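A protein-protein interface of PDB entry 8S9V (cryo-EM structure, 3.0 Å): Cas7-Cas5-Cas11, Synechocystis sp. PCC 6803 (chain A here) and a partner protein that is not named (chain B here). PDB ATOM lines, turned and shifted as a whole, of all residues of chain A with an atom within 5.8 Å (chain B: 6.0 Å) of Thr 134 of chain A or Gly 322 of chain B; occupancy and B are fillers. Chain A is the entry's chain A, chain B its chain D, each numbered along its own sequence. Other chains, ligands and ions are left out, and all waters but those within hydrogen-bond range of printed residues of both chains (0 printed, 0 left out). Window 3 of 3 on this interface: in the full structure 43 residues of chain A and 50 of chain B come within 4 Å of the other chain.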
ATOM      1  N   ASP A 131      19.018  22.947 -11.122  1.00  0.00           N
ATOM      2  CA  ASP A 131      18.227  21.812 -10.678  1.00  0.00           C
ATOM      3  C   ASP A 131      17.076  22.261  -9.797  1.00  0.00           C
ATOM      4  O   ASP A 131      17.283  22.904  -8.772  1.00  0.00           O
ATOM      5  CB  ASP A 131      19.134  20.838  -9.942  1.00  0.00           C
ATOM      6  CG  ASP A 131      18.391  19.658  -9.386  1.00  0.00           C
ATOM      7  OD1 ASP A 131      17.292  19.842  -8.829  1.00  0.00           O
ATOM      8  OD2 ASP A 131      18.900  18.530  -9.525  1.00  0.00           O
ATOM      9  N   ALA A 132      15.863  21.894 -10.187  1.00  0.00           N
ATOM     10  CA  ALA A 132      14.676  22.418  -9.528  1.00  0.00           C
ATOM     11  C   ALA A 132      14.520  21.969  -8.081  1.00  0.00           C
ATOM     12  O   ALA A 132      13.992  22.735  -7.270  1.00  0.00           O
ATOM     13  CB  ALA A 132      13.435  22.024 -10.317  1.00  0.00           C
ATOM     14  N   ILE A 133      14.949  20.767  -7.713  1.00  0.00           N
ATOM     15  CA  ILE A 133      14.750  20.369  -6.319  1.00  0.00           C
ATOM     16  C   ILE A 133      15.861  20.856  -5.398  1.00  0.00           C
ATOM     17  O   ILE A 133      15.581  21.372  -4.317  1.00  0.00           O
ATOM     18  CB  ILE A 133      14.581  18.845  -6.233  1.00  0.00           C
ATOM     19  CG1 ILE A 133      15.828  18.143  -6.741  1.00  0.00           C
ATOM     20  CG2 ILE A 133      13.399  18.407  -7.027  1.00  0.00           C
ATOM     21  CD1 ILE A 133      15.875  16.675  -6.407  1.00  0.00           C
ATOM     22  N   THR A 134      17.126  20.736  -5.796  1.00  0.00           N
ATOM     23  CA  THR A 134      18.231  21.216  -4.975  1.00  0.00           C
ATOM     24  C   THR A 134      18.469  22.710  -5.089  1.00  0.00           C
ATOM     25  O   THR A 134      19.024  23.299  -4.169  1.00  0.00           O
ATOM     26  CB  THR A 134      19.494  20.467  -5.332  1.00  0.00           C
ATOM     27  OG1 THR A 134      19.872  20.817  -6.657  1.00  0.00           O
ATOM     28  CG2 THR A 134      19.245  19.019  -5.276  1.00  0.00           C
ATOM     29  N   GLY A 135      18.051  23.343  -6.172  1.00  0.00           N
ATOM     30  CA  GLY A 135      18.366  24.734  -6.387  1.00  0.00           C
ATOM     31  C   GLY A 135      19.794  25.072  -6.721  1.00  0.00           C
ATOM     32  O   GLY A 135      20.183  26.223  -6.555  1.00  0.00           O
ATOM     33  N   THR A 136      20.585  24.120  -7.206  1.00  0.00           N
ATOM     34  CA  THR A 136      21.983  24.351  -7.546  1.00  0.00           C
ATOM     35  C   THR A 136      22.202  24.005  -9.017  1.00  0.00           C
ATOM     36  O   THR A 136      21.455  23.236  -9.608  1.00  0.00           O
ATOM     37  CB  THR A 136      22.949  23.557  -6.654  1.00  0.00           C
ATOM     38  OG1 THR A 136      22.768  22.160  -6.854  1.00  0.00           O
ATOM     39  CG2 THR A 136      22.670  23.833  -5.244  1.00  0.00           C
ATOM     40  N   SER B 307      24.390  23.474   1.361  1.00  0.00           N
ATOM     41  CA  SER B 307      25.729  22.989   1.099  1.00  0.00           C
ATOM     42  C   SER B 307      26.215  23.445  -0.267  1.00  0.00           C
ATOM     43  O   SER B 307      25.431  23.682  -1.180  1.00  0.00           O
ATOM     44  CB  SER B 307      25.801  21.478   1.234  1.00  0.00           C
ATOM     45  OG  SER B 307      24.920  20.830   0.355  1.00  0.00           O
ATOM     46  N   ALA B 308      27.529  23.552  -0.394  1.00  0.00           N
ATOM     47  CA  ALA B 308      28.151  23.902  -1.654  1.00  0.00           C
ATOM     48  C   ALA B 308      27.866  22.840  -2.686  1.00  0.00           C
ATOM     49  O   ALA B 308      27.807  21.656  -2.370  1.00  0.00           O
ATOM     50  CB  ALA B 308      29.649  24.046  -1.473  1.00  0.00           C
ATOM     51  N   SER B 309      27.711  23.255  -3.931  1.00  0.00           N
ATOM     52  CA  SER B 309      27.739  22.294  -5.017  1.00  0.00           C
ATOM     53  C   SER B 309      29.065  21.562  -5.041  1.00  0.00           C
ATOM     54  O   SER B 309      30.122  22.156  -4.848  1.00  0.00           O
ATOM     55  CB  SER B 309      27.533  22.999  -6.344  1.00  0.00           C
ATOM     56  OG  SER B 309      26.182  23.299  -6.558  1.00  0.00           O
ATOM     57  N   LEU B 310      29.005  20.250  -5.212  1.00  0.00           N
ATOM     58  CA  LEU B 310      30.217  19.445  -5.284  1.00  0.00           C
ATOM     59  C   LEU B 310      29.823  18.131  -5.935  1.00  0.00           C
ATOM     60  O   LEU B 310      29.189  17.300  -5.289  1.00  0.00           O
ATOM     61  CB  LEU B 310      30.805  19.233  -3.909  1.00  0.00           C
ATOM     62  CG  LEU B 310      31.905  18.196  -3.847  1.00  0.00           C
ATOM     63  CD1 LEU B 310      32.975  18.575  -4.796  1.00  0.00           C
ATOM     64  CD2 LEU B 310      32.448  18.095  -2.464  1.00  0.00           C
ATOM     65  N   ASP B 320      25.586  15.127  -7.176  1.00  0.00           N
ATOM     66  CA  ASP B 320      25.888  16.415  -6.577  1.00  0.00           C
ATOM     67  C   ASP B 320      25.494  16.467  -5.103  1.00  0.00           C
ATOM     68  O   ASP B 320      24.351  16.180  -4.752  1.00  0.00           O
ATOM     69  CB  ASP B 320      25.202  17.510  -7.388  1.00  0.00           C
ATOM     70  CG  ASP B 320      25.507  18.879  -6.880  1.00  0.00           C
ATOM     71  OD1 ASP B 320      26.484  19.016  -6.126  1.00  0.00           O
ATOM     72  OD2 ASP B 320      24.786  19.825  -7.251  1.00  0.00           O
ATOM     73  N   LEU B 321      26.452  16.809  -4.248  1.00  0.00           N
ATOM     74  CA  LEU B 321      26.225  17.095  -2.836  1.00  0.00           C
ATOM     75  C   LEU B 321      25.592  18.454  -2.560  1.00  0.00           C
ATOM     76  O   LEU B 321      25.161  18.697  -1.431  1.00  0.00           O
ATOM     77  CB  LEU B 321      27.541  17.034  -2.066  1.00  0.00           C
ATOM     78  CG  LEU B 321      28.094  15.715  -1.559  1.00  0.00           C
ATOM     79  CD1 LEU B 321      28.386  14.795  -2.707  1.00  0.00           C
ATOM     80  CD2 LEU B 321      29.326  15.970  -0.750  1.00  0.00           C
ATOM     81  N   GLY B 322      25.545  19.351  -3.534  1.00  0.00           N
ATOM     82  CA  GLY B 322      25.051  20.686  -3.282  1.00  0.00           C
ATOM     83  C   GLY B 322      23.546  20.771  -3.162  1.00  0.00           C
ATOM     84  O   GLY B 322      22.804  20.180  -3.936  1.00  0.00           O
ATOM     85  N   LYS B 323      23.100  21.528  -2.168  1.00  0.00           N
ATOM     86  CA  LYS B 323      21.720  21.960  -2.116  1.00  0.00           C
ATOM     87  C   LYS B 323      21.607  23.327  -1.469  1.00  0.00           C
ATOM     88  O   LYS B 323      22.383  23.678  -0.588  1.00  0.00           O
ATOM     89  CB  LYS B 323      20.861  20.959  -1.365  1.00  0.00           C
ATOM     90  CG  LYS B 323      21.142  20.851   0.077  1.00  0.00           C
ATOM     91  CD  LYS B 323      20.477  19.625   0.596  1.00  0.00           C
ATOM     92  CE  LYS B 323      21.111  18.385   0.084  1.00  0.00           C
ATOM     93  NZ  LYS B 323      20.335  17.232   0.549  1.00  0.00           N
ATOM     94  N   ILE B 324      20.634  24.098  -1.943  1.00  0.00           N
ATOM     95  CA  ILE B 324      20.375  25.429  -1.426  1.00  0.00           C
ATOM     96  C   ILE B 324      19.867  25.345   0.004  1.00  0.00           C
ATOM     97  O   ILE B 324      19.245  24.367   0.410  1.00  0.00           O
ATOM     98  CB  ILE B 324      19.366  26.129  -2.344  1.00  0.00           C
ATOM     99  CG1 ILE B 324      19.256  27.600  -2.030  1.00  0.00           C
ATOM    100  CG2 ILE B 324      18.073  25.540  -2.131  1.00  0.00           C
ATOM    101  CD1 ILE B 324      18.555  28.358  -3.057  1.00  0.00           C
ATOM    102  N   GLY B 325      20.129  26.386   0.782  1.00  0.00           N
ATOM    103  CA  GLY B 325      19.563  26.473   2.116  1.00  0.00           C
ATOM    104  C   GLY B 325      18.060  26.618   2.100  1.00  0.00           C
ATOM    105  O   GLY B 325      17.517  27.531   1.474  1.00  0.00           O
ATOM    106  N   ARG B 419      10.805  23.370   0.626  1.00  0.00           N
ATOM    107  CA  ARG B 419      12.131  22.927   0.203  1.00  0.00           C
ATOM    108  C   ARG B 419      12.698  21.806   1.063  1.00  0.00           C
ATOM    109  O   ARG B 419      13.246  20.846   0.526  1.00  0.00           O
ATOM    110  CB  ARG B 419      13.072  24.129   0.222  1.00  0.00           C
ATOM    111  CG  ARG B 419      14.496  23.914  -0.230  1.00  0.00           C
ATOM    112  CD  ARG B 419      14.717  23.302  -1.589  1.00  0.00           C
ATOM    113  NE  ARG B 419      14.175  24.039  -2.702  1.00  0.00           N
ATOM    114  CZ  ARG B 419      14.522  25.262  -3.065  1.00  0.00           C
ATOM    115  NH1 ARG B 419      14.267  25.700  -4.273  1.00  0.00           N
ATOM    116  NH2 ARG B 419      15.273  25.980  -2.258  1.00  0.00           N
ATOM    117  N   TYR B 423      13.473  17.868   0.007  1.00  0.00           N
ATOM    118  CA  TYR B 423      14.709  17.146   0.305  1.00  0.00           C
ATOM    119  C   TYR B 423      14.431  15.815   0.961  1.00  0.00           C
ATOM    120  O   TYR B 423      15.114  14.831   0.681  1.00  0.00           O
ATOM    121  CB  TYR B 423      15.628  17.944   1.224  1.00  0.00           C
ATOM    122  CG  TYR B 423      16.173  19.235   0.704  1.00  0.00           C
ATOM    123  CD1 TYR B 423      16.302  19.470  -0.638  1.00  0.00           C
ATOM    124  CD2 TYR B 423      16.604  20.199   1.562  1.00  0.00           C
ATOM    125  CE1 TYR B 423      16.820  20.629  -1.090  1.00  0.00           C
ATOM    126  CE2 TYR B 423      17.111  21.358   1.105  1.00  0.00           C
ATOM    127  CZ  TYR B 423      17.219  21.564  -0.208  1.00  0.00           C
ATOM    128  OH  TYR B 423      17.727  22.735  -0.643  1.00  0.00           O
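OD2 of Asp 320 of chain B sits at hydrogen-bond distance from OG1 of Thr 136 of chain A.
N of Ile 324 of chain B sits at hydrogen-bond distance from O of Thr 134 of chain A (2.9 Å).
The backbone carbonyl oxygen (O) of Ile 133 of chain A is in hydrogen-bond range of the guanidinium group (NE) of Arg 419 of chain B (3.4 Å).
Of chain B, only Gly 322 (3.6 Å), Lys 323 (3.6 Å), Ile 324 (2.9 Å) and Tyr 423 (3.8 Å) come within 4 Å of Thr 134 of chain A.
Printed residues of chain A within 4 Å of Ser 309 of chain B: Thr 136.
Gly 322 of chain B touches just these residues of chain A: Thr 134 and Thr 136.
Of the printed residues of chain A, Lys 323 of chain B touches Thr 134 (3.6 Å) and Thr 136 (3.8 Å).
The nearest printed residue of chain A that does not touch Gly 322 of chain B is Gly 135 of chain A (6.1 Å).
The nearest printed residue of chain A that does not touch Ile 324 of chain B is Gly 135 of chain A (4.3 Å).
Tyr 423 of chain B touches Ile 133 of chain A.
O of Gly 322 of chain B touches CB of Thr 134 of chain A, at 3.6 Å.
Thr 134 of chain A touches Lys 323 of chain B.
Thr 134 of chain A touches Tyr 423 of chain B (O to OH, 3.8 Å).
CB of Thr 136 of chain A touches OG of Ser 309 of chain B (3.2 Å).
Thr 136 of chain A touches Gly 322 of chain B (OG1 to O, 3.5 Å).
Lys 323 of chain B touches Thr 136 of chain A.
N of Ile 324 of chain B touches CG2 of Thr 136 of chain A (3.9 Å).
OG1 of Thr 134 of chain A sits at hydrogen-bond distance from OG1 of Thr 136 of chain A (3.2 Å).
The side-chain hydroxyl of Tyr 423 of chain B is in hydrogen-bond range of the backbone carbonyl oxygen of Ile 324 of chain B (2.5 Å).
The backbone NH (N) of Ser 307 of chain B sits at hydrogen-bond distance from the backbone carbonyl oxygen (O) of Lys 323 of chain B, at 2.8 Å.
The side-chain carboxylate of Asp 131 of chain A sits at hydrogen-bond distance from the backbone NH of Ile 133 of chain A (2.8 Å).
The side-chain carboxylate (OD1) of Asp 320 of chain B sits at hydrogen-bond distance from the backbone NH (N) of Gly 322 of chain B, at 2.8 Å.
O of Thr 136 of chain A lies within hydrogen-bond range of N of Asp 131 of chain A (2.9 Å).
Of the 6 printed residues of chain A, 3 touch a printed residue of chain B.
Hydrophobic or aromatic side chains of chain B that line the printed part of chain A: Ile 324 and Tyr 423.
Among the printed residues, 11 pairs touch across the chains.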
